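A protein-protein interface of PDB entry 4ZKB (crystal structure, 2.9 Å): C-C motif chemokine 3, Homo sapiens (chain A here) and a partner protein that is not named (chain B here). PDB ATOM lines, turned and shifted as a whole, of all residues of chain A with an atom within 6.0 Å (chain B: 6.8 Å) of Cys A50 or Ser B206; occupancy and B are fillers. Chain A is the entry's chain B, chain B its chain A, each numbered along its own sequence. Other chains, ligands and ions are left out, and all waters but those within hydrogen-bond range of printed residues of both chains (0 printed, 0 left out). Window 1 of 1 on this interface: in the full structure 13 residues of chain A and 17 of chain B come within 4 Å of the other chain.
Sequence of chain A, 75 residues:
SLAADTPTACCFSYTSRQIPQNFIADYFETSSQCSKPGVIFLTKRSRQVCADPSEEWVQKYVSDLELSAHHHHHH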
ATOM      1  N   CYS A  10     -11.703  -8.493 -14.271  1.00  0.00           N
ATOM      2  CA  CYS A  10     -11.098  -9.366 -13.284  1.00  0.00           C
ATOM      3  C   CYS A  10     -10.533 -10.587 -13.934  1.00  0.00           C
ATOM      4  O   CYS A  10     -11.260 -11.432 -14.424  1.00  0.00           O
ATOM      5  CB  CYS A  10     -12.098  -9.758 -12.222  1.00  0.00           C
ATOM      6  SG  CYS A  10     -11.868  -8.728 -10.776  1.00  0.00           S
ATOM      7  N   CYS A  11      -9.218 -10.685 -13.922  1.00  0.00           N
ATOM      8  CA  CYS A  11      -8.563 -11.654 -14.751  1.00  0.00           C
ATOM      9  C   CYS A  11      -8.450 -13.021 -14.099  1.00  0.00           C
ATOM     10  O   CYS A  11      -7.884 -13.149 -13.013  1.00  0.00           O
ATOM     11  CB  CYS A  11      -7.198 -11.150 -15.163  1.00  0.00           C
ATOM     12  SG  CYS A  11      -6.823 -11.974 -16.699  1.00  0.00           S
ATOM     13  N   PHE A  12      -8.998 -14.031 -14.779  1.00  0.00           N
ATOM     14  CA  PHE A  12      -9.042 -15.409 -14.274  1.00  0.00           C
ATOM     15  C   PHE A  12      -7.932 -16.285 -14.869  1.00  0.00           C
ATOM     16  O   PHE A  12      -7.568 -17.299 -14.279  1.00  0.00           O
ATOM     17  CB  PHE A  12     -10.401 -16.056 -14.582  1.00  0.00           C
ATOM     18  CG  PHE A  12     -11.554 -15.556 -13.731  1.00  0.00           C
ATOM     19  CD1 PHE A  12     -12.643 -16.391 -13.472  1.00  0.00           C
ATOM     20  CD2 PHE A  12     -11.576 -14.261 -13.204  1.00  0.00           C
ATOM     21  CE1 PHE A  12     -13.716 -15.949 -12.712  1.00  0.00           C
ATOM     22  CE2 PHE A  12     -12.647 -13.818 -12.440  1.00  0.00           C
ATOM     23  CZ  PHE A  12     -13.715 -14.664 -12.191  1.00  0.00           C
ATOM     24  N   SER A  13      -7.418 -15.921 -16.041  1.00  0.00           N
ATOM     25  CA  SER A  13      -6.281 -16.635 -16.629  1.00  0.00           C
ATOM     26  C   SER A  13      -5.396 -15.696 -17.446  1.00  0.00           C
ATOM     27  O   SER A  13      -5.888 -14.882 -18.235  1.00  0.00           O
ATOM     28  CB  SER A  13      -6.747 -17.804 -17.502  1.00  0.00           C
ATOM     29  OG  SER A  13      -5.659 -18.654 -17.841  1.00  0.00           O
ATOM     30  N   TYR A  14      -4.089 -15.816 -17.244  1.00  0.00           N
ATOM     31  CA  TYR A  14      -3.127 -14.959 -17.912  1.00  0.00           C
ATOM     32  C   TYR A  14      -2.604 -15.657 -19.175  1.00  0.00           C
ATOM     33  O   TYR A  14      -2.797 -16.866 -19.359  1.00  0.00           O
ATOM     34  CB  TYR A  14      -1.987 -14.618 -16.946  1.00  0.00           C
ATOM     35  N   THR A  15      -1.980 -14.885 -20.063  1.00  0.00           N
ATOM     36  CA  THR A  15      -1.265 -15.473 -21.191  1.00  0.00           C
ATOM     37  C   THR A  15       0.121 -15.828 -20.716  1.00  0.00           C
ATOM     38  O   THR A  15       0.729 -15.039 -20.001  1.00  0.00           O
ATOM     39  CB  THR A  15      -1.154 -14.520 -22.386  1.00  0.00           C
ATOM     40  OG1 THR A  15      -0.555 -15.218 -23.481  1.00  0.00           O
ATOM     41  CG2 THR A  15      -0.301 -13.301 -22.059  1.00  0.00           C
ATOM     42  N   SER A  16       0.613 -17.009 -21.099  1.00  0.00           N
ATOM     43  CA  SER A  16       1.954 -17.481 -20.689  1.00  0.00           C
ATOM     44  C   SER A  16       3.069 -16.723 -21.401  1.00  0.00           C
ATOM     45  O   SER A  16       4.079 -16.383 -20.793  1.00  0.00           O
ATOM     46  CB  SER A  16       2.113 -18.985 -20.952  1.00  0.00           C
ATOM     47  OG  SER A  16       1.102 -19.739 -20.298  1.00  0.00           O
ATOM     48  N   VAL A  39      -2.566  -7.538 -15.017  1.00  0.00           N
ATOM     49  CA  VAL A  39      -2.464  -6.392 -15.896  1.00  0.00           C
ATOM     50  C   VAL A  39      -3.193  -6.718 -17.194  1.00  0.00           C
ATOM     51  O   VAL A  39      -2.691  -7.462 -18.029  1.00  0.00           O
ATOM     52  CB  VAL A  39      -0.996  -6.016 -16.188  1.00  0.00           C
ATOM     53  N   ILE A  40      -4.402  -6.189 -17.339  1.00  0.00           N
ATOM     54  CA  ILE A  40      -5.072  -6.184 -18.630  1.00  0.00           C
ATOM     55  C   ILE A  40      -4.262  -5.250 -19.533  1.00  0.00           C
ATOM     56  O   ILE A  40      -3.863  -4.157 -19.115  1.00  0.00           O
ATOM     57  CB  ILE A  40      -6.541  -5.716 -18.527  1.00  0.00           C
ATOM     58  N   PHE A  41      -3.985  -5.707 -20.749  1.00  0.00           N
ATOM     59  CA  PHE A  41      -3.223  -4.950 -21.722  1.00  0.00           C
ATOM     60  C   PHE A  41      -4.083  -4.761 -22.961  1.00  0.00           C
ATOM     61  O   PHE A  41      -4.576  -5.745 -23.550  1.00  0.00           O
ATOM     62  CB  PHE A  41      -1.934  -5.689 -22.086  1.00  0.00           C
ATOM     63  N   GLN A  48      -7.846  -7.544 -25.914  1.00  0.00           N
ATOM     64  CA  GLN A  48      -7.511  -7.009 -24.602  1.00  0.00           C
ATOM     65  C   GLN A  48      -6.940  -8.208 -23.836  1.00  0.00           C
ATOM     66  O   GLN A  48      -7.700  -9.040 -23.337  1.00  0.00           O
ATOM     67  CB  GLN A  48      -8.787  -6.484 -23.937  1.00  0.00           C
ATOM     68  CG  GLN A  48      -8.603  -5.325 -22.966  1.00  0.00           C
ATOM     69  CD  GLN A  48      -9.928  -4.674 -22.551  1.00  0.00           C
ATOM     70  OE1 GLN A  48     -10.186  -4.469 -21.367  1.00  0.00           O
ATOM     71  NE2 GLN A  48     -10.767  -4.343 -23.531  1.00  0.00           N
ATOM     72  N   VAL A  49      -5.615  -8.339 -23.786  1.00  0.00           N
ATOM     73  CA  VAL A  49      -5.014  -9.603 -23.324  1.00  0.00           C
ATOM     74  C   VAL A  49      -4.522  -9.479 -21.898  1.00  0.00           C
ATOM     75  O   VAL A  49      -4.144  -8.406 -21.459  1.00  0.00           O
ATOM     76  CB  VAL A  49      -3.851 -10.061 -24.218  1.00  0.00           C
ATOM     77  N   CYS A  50      -4.498 -10.598 -21.194  1.00  0.00           N
ATOM     78  CA  CYS A  50      -4.264 -10.603 -19.761  1.00  0.00           C
ATOM     79  C   CYS A  50      -2.911 -11.188 -19.366  1.00  0.00           C
ATOM     80  O   CYS A  50      -2.421 -12.121 -20.009  1.00  0.00           O
ATOM     81  CB  CYS A  50      -5.367 -11.404 -19.107  1.00  0.00           C
ATOM     82  SG  CYS A  50      -6.487 -10.496 -18.025  1.00  0.00           S
ATOM     83  N   ALA A  51      -2.359 -10.666 -18.263  1.00  0.00           N
ATOM     84  CA  ALA A  51      -0.962 -10.896 -17.852  1.00  0.00           C
ATOM     85  C   ALA A  51      -0.802 -11.256 -16.354  1.00  0.00           C
ATOM     86  O   ALA A  51      -1.792 -11.294 -15.615  1.00  0.00           O
ATOM     87  CB  ALA A  51      -0.150  -9.653 -18.175  1.00  0.00           C
ATOM     88  N   ASP A  52       0.442 -11.529 -15.933  1.00  0.00           N
ATOM     89  CA  ASP A  52       0.804 -11.805 -14.517  1.00  0.00           C
ATOM     90  C   ASP A  52       1.916 -10.861 -14.031  1.00  0.00           C
ATOM     91  O   ASP A  52       2.167  -9.826 -14.649  1.00  0.00           O
ATOM     92  CB  ASP A  52       1.259 -13.263 -14.344  1.00  0.00           C
ATOM     93  N   LEU B 143      -2.749 -17.767 -29.734  1.00  0.00           N
ATOM     94  CA  LEU B 143      -3.391 -17.237 -28.523  1.00  0.00           C
ATOM     95  C   LEU B 143      -4.895 -17.411 -28.563  1.00  0.00           C
ATOM     96  O   LEU B 143      -5.529 -17.239 -29.617  1.00  0.00           O
ATOM     97  CB  LEU B 143      -3.090 -15.753 -28.333  1.00  0.00           C
ATOM     98  CG  LEU B 143      -3.835 -15.073 -27.169  1.00  0.00           C
ATOM     99  CD1 LEU B 143      -3.179 -15.387 -25.828  1.00  0.00           C
ATOM    100  CD2 LEU B 143      -3.920 -13.570 -27.378  1.00  0.00           C
ATOM    101  N   LEU B 144      -5.454 -17.729 -27.395  1.00  0.00           N
ATOM    102  CA  LEU B 144      -6.900 -17.776 -27.208  1.00  0.00           C
ATOM    103  C   LEU B 144      -7.313 -16.673 -26.248  1.00  0.00           C
ATOM    104  O   LEU B 144      -6.871 -16.655 -25.109  1.00  0.00           O
ATOM    105  CB  LEU B 144      -7.318 -19.138 -26.645  1.00  0.00           C
ATOM    106  CG  LEU B 144      -8.778 -19.293 -26.214  1.00  0.00           C
ATOM    107  CD1 LEU B 144      -9.702 -18.933 -27.350  1.00  0.00           C
ATOM    108  CD2 LEU B 144      -9.058 -20.710 -25.764  1.00  0.00           C
ATOM    109  N   ALA B 145      -8.158 -15.754 -26.702  1.00  0.00           N
ATOM    110  CA  ALA B 145      -8.658 -14.701 -25.821  1.00  0.00           C
ATOM    111  C   ALA B 145     -10.147 -14.852 -25.610  1.00  0.00           C
ATOM    112  O   ALA B 145     -10.918 -14.767 -26.568  1.00  0.00           O
ATOM    113  CB  ALA B 145      -8.373 -13.339 -26.410  1.00  0.00           C
ATOM    114  N   ILE B 146     -10.549 -15.068 -24.360  1.00  0.00           N
ATOM    115  CA  ILE B 146     -11.959 -15.151 -24.015  1.00  0.00           C
ATOM    116  C   ILE B 146     -12.297 -14.030 -23.071  1.00  0.00           C
ATOM    117  O   ILE B 146     -11.680 -13.900 -22.014  1.00  0.00           O
ATOM    118  CB  ILE B 146     -12.294 -16.452 -23.295  1.00  0.00           C
ATOM    119  CG1 ILE B 146     -12.031 -17.636 -24.210  1.00  0.00           C
ATOM    120  CG2 ILE B 146     -13.746 -16.447 -22.863  1.00  0.00           C
ATOM    121  CD1 ILE B 146     -11.945 -18.948 -23.466  1.00  0.00           C
ATOM    122  N   GLN B 147     -13.291 -13.238 -23.446  1.00  0.00           N
ATOM    123  CA  GLN B 147     -13.696 -12.114 -22.622  1.00  0.00           C
ATOM    124  C   GLN B 147     -15.189 -12.179 -22.363  1.00  0.00           C
ATOM    125  O   GLN B 147     -15.940 -12.576 -23.221  1.00  0.00           O
ATOM    126  CB  GLN B 147     -13.340 -10.814 -23.313  1.00  0.00           C
ATOM    127  CG  GLN B 147     -13.269  -9.637 -22.366  1.00  0.00           C
ATOM    128  CD  GLN B 147     -13.039  -8.324 -23.095  1.00  0.00           C
ATOM    129  OE1 GLN B 147     -12.064  -8.178 -23.838  1.00  0.00           O
ATOM    130  NE2 GLN B 147     -13.931  -7.361 -22.885  1.00  0.00           N
ATOM    131  N   ASP B 204      -2.652 -21.663 -24.792  1.00  0.00           N
ATOM    132  CA  ASP B 204      -2.393 -20.354 -24.202  1.00  0.00           C
ATOM    133  C   ASP B 204      -3.639 -19.475 -24.300  1.00  0.00           C
ATOM    134  O   ASP B 204      -3.912 -18.867 -25.348  1.00  0.00           O
ATOM    135  CB  ASP B 204      -1.209 -19.695 -24.911  1.00  0.00           C
ATOM    136  CG  ASP B 204      -0.741 -18.428 -24.225  1.00  0.00           C
ATOM    137  OD1 ASP B 204      -0.900 -18.308 -22.990  1.00  0.00           O
ATOM    138  OD2 ASP B 204      -0.199 -17.553 -24.932  1.00  0.00           O
ATOM    139  N   PHE B 205      -4.411 -19.417 -23.217  1.00  0.00           N
ATOM    140  CA  PHE B 205      -5.596 -18.566 -23.206  1.00  0.00           C
ATOM    141  C   PHE B 205      -5.557 -17.505 -22.111  1.00  0.00           C
ATOM    142  O   PHE B 205      -5.098 -17.757 -21.002  1.00  0.00           O
ATOM    143  CB  PHE B 205      -6.885 -19.391 -23.145  1.00  0.00           C
ATOM    144  CG  PHE B 205      -7.075 -20.148 -21.867  1.00  0.00           C
ATOM    145  CD1 PHE B 205      -6.702 -21.488 -21.769  1.00  0.00           C
ATOM    146  CD2 PHE B 205      -7.656 -19.542 -20.767  1.00  0.00           C
ATOM    147  CE1 PHE B 205      -6.891 -22.196 -20.593  1.00  0.00           C
ATOM    148  CE2 PHE B 205      -7.837 -20.242 -19.584  1.00  0.00           C
ATOM    149  CZ  PHE B 205      -7.456 -21.570 -19.497  1.00  0.00           C
ATOM    150  N   SER B 206      -5.987 -16.302 -22.476  1.00  0.00           N
ATOM    151  CA  SER B 206      -6.371 -15.290 -21.519  1.00  0.00           C
ATOM    152  C   SER B 206      -7.877 -15.329 -21.357  1.00  0.00           C
ATOM    153  O   SER B 206      -8.632 -15.320 -22.334  1.00  0.00           O
ATOM    154  CB  SER B 206      -5.985 -13.894 -21.970  1.00  0.00           C
ATOM    155  OG  SER B 206      -6.770 -12.927 -21.275  1.00  0.00           O
ATOM    156  N   LEU B 207      -8.294 -15.350 -20.099  1.00  0.00           N
ATOM    157  CA  LEU B 207      -9.690 -15.418 -19.728  1.00  0.00           C
ATOM    158  C   LEU B 207     -10.024 -14.202 -18.862  1.00  0.00           C
ATOM    159  O   LEU B 207      -9.575 -14.092 -17.711  1.00  0.00           O
ATOM    160  CB  LEU B 207      -9.941 -16.716 -18.973  1.00  0.00           C
ATOM    161  CG  LEU B 207     -11.327 -16.895 -18.365  1.00  0.00           C
ATOM    162  CD1 LEU B 207     -12.409 -16.512 -19.358  1.00  0.00           C
ATOM    163  CD2 LEU B 207     -11.504 -18.326 -17.880  1.00  0.00           C
ATOM    164  N   LEU B 208     -10.798 -13.285 -19.429  1.00  0.00           N
ATOM    165  CA  LEU B 208     -11.111 -12.044 -18.760  1.00  0.00           C
ATOM    166  C   LEU B 208     -12.620 -11.911 -18.570  1.00  0.00           C
ATOM    167  O   LEU B 208     -13.378 -12.109 -19.515  1.00  0.00           O
ATOM    168  CB  LEU B 208     -10.565 -10.891 -19.588  1.00  0.00           C
ATOM    169  CG  LEU B 208     -10.960  -9.487 -19.134  1.00  0.00           C
ATOM    170  CD1 LEU B 208     -10.668  -9.281 -17.656  1.00  0.00           C
ATOM    171  CD2 LEU B 208     -10.246  -8.430 -19.965  1.00  0.00           C
ATOM    172  N   VAL B 209     -13.055 -11.587 -17.350  1.00  0.00           N
ATOM    173  CA  VAL B 209     -14.482 -11.480 -17.040  1.00  0.00           C
ATOM    174  C   VAL B 209     -14.860 -10.328 -16.115  1.00  0.00           C
ATOM    175  O   VAL B 209     -14.030  -9.760 -15.428  1.00  0.00           O
ATOM    176  CB  VAL B 209     -15.006 -12.765 -16.371  1.00  0.00           C
ATOM    177  CG1 VAL B 209     -14.572 -13.989 -17.162  1.00  0.00           C
ATOM    178  CG2 VAL B 209     -14.544 -12.865 -14.923  1.00  0.00           C
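SG of Cys A50 is disulfide-bonded to SG of Cys A11. The backbone NH (N) of Ile B146 lies within hydrogen-bond range of the backbone carbonyl oxygen (O) of Ser B206, 2.8 Å away. N of Thr A15 sits at hydrogen-bond distance from O of Cys A50, at 2.8 Å. The backbone carbonyl oxygen of Ile B146 is in hydrogen-bond range of the backbone NH of Leu B208. The backbone carbonyl oxygen (O) of Leu B144 is in hydrogen-bond range of the backbone NH (N) of Ser B206 (2.8 Å). The backbone NH (N) of Leu B144 is in hydrogen-bond range of the backbone carbonyl oxygen (O) of Asp B204, 2.8 Å away.
Among the printed residues, merely in contact across the chains: Cys A10 with Leu B208 (3.6 Å), Phe A12 with Val B209 (3.3 Å), Ser A13 with Ser B206 (3.3 Å), Thr A15 with Leu B143 (3.5 Å) and Gln A48 with Gln B147 (3.7 Å).
Printed residues of chain B that touch a printed residue of chain A: Leu B143, Gln B147, Asp B204, Phe B205, Ser B206, Leu B207, Leu B208 and Val B209. Hydrophobic or aromatic side chains of chain B that line the printed part of chain A: Leu B143, Phe B205, Leu B207, Leu B208 and Val B209. Hydrophobic or aromatic side chains of chain A within 4 Å of the printed part of chain B: Phe A12. Among the printed residues, 14 pairs touch across the chains. Among the printed residues, no Asp or Glu carboxylate lies within 4 Å of a Lys or Arg side-chain nitrogen of the other chain.
The backbone NH of Leu B207 sits at hydrogen-bond distance from the backbone carbonyl oxygen of Ser A13. The backbone carbonyl oxygen (O) of Val B209 lies within hydrogen-bond range of the backbone NH (N) of Cys A10 (2.9 Å). The backbone carbonyl oxygen of Phe B205 lies close to the side-chain hydroxyl of Ser A13 (3.3 Å). The side-chain carboxylate (OD2) of Asp B204 lies within hydrogen-bond range of the side-chain hydroxyl (OG1) of Thr A15 (2.8 Å). The backbone NH (N) of Cys A50 sits close to the side-chain hydroxyl (OG) of Ser B206 (3.3 Å). The side-chain sulfur (SG) of Cys A11 sits close to the backbone carbonyl oxygen (O) of Leu B207, 3.6 Å away. N of Ser A16 sits at hydrogen-bond distance from OD1 of Asp B204 (2.7 Å). O of Tyr A14 sits close to O of Phe B205, 3.0 Å away. O of Leu B207 sits at hydrogen-bond distance from N of Phe A12 (3.0 Å).
Of the printed residues of chain B, Thr A15 touches Leu B143 (3.5 Å) and Asp B204 (2.8 Å). Of chain B, only Ser B206 comes within 4 Å of Cys A50. Ala A51 touches none of the printed residues of chain B. Of the printed residues of chain A, Gln B147 touches Gln A48. The nearest printed residue of chain B that does not touch Ser A16 is Phe B205 (5.8 Å).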
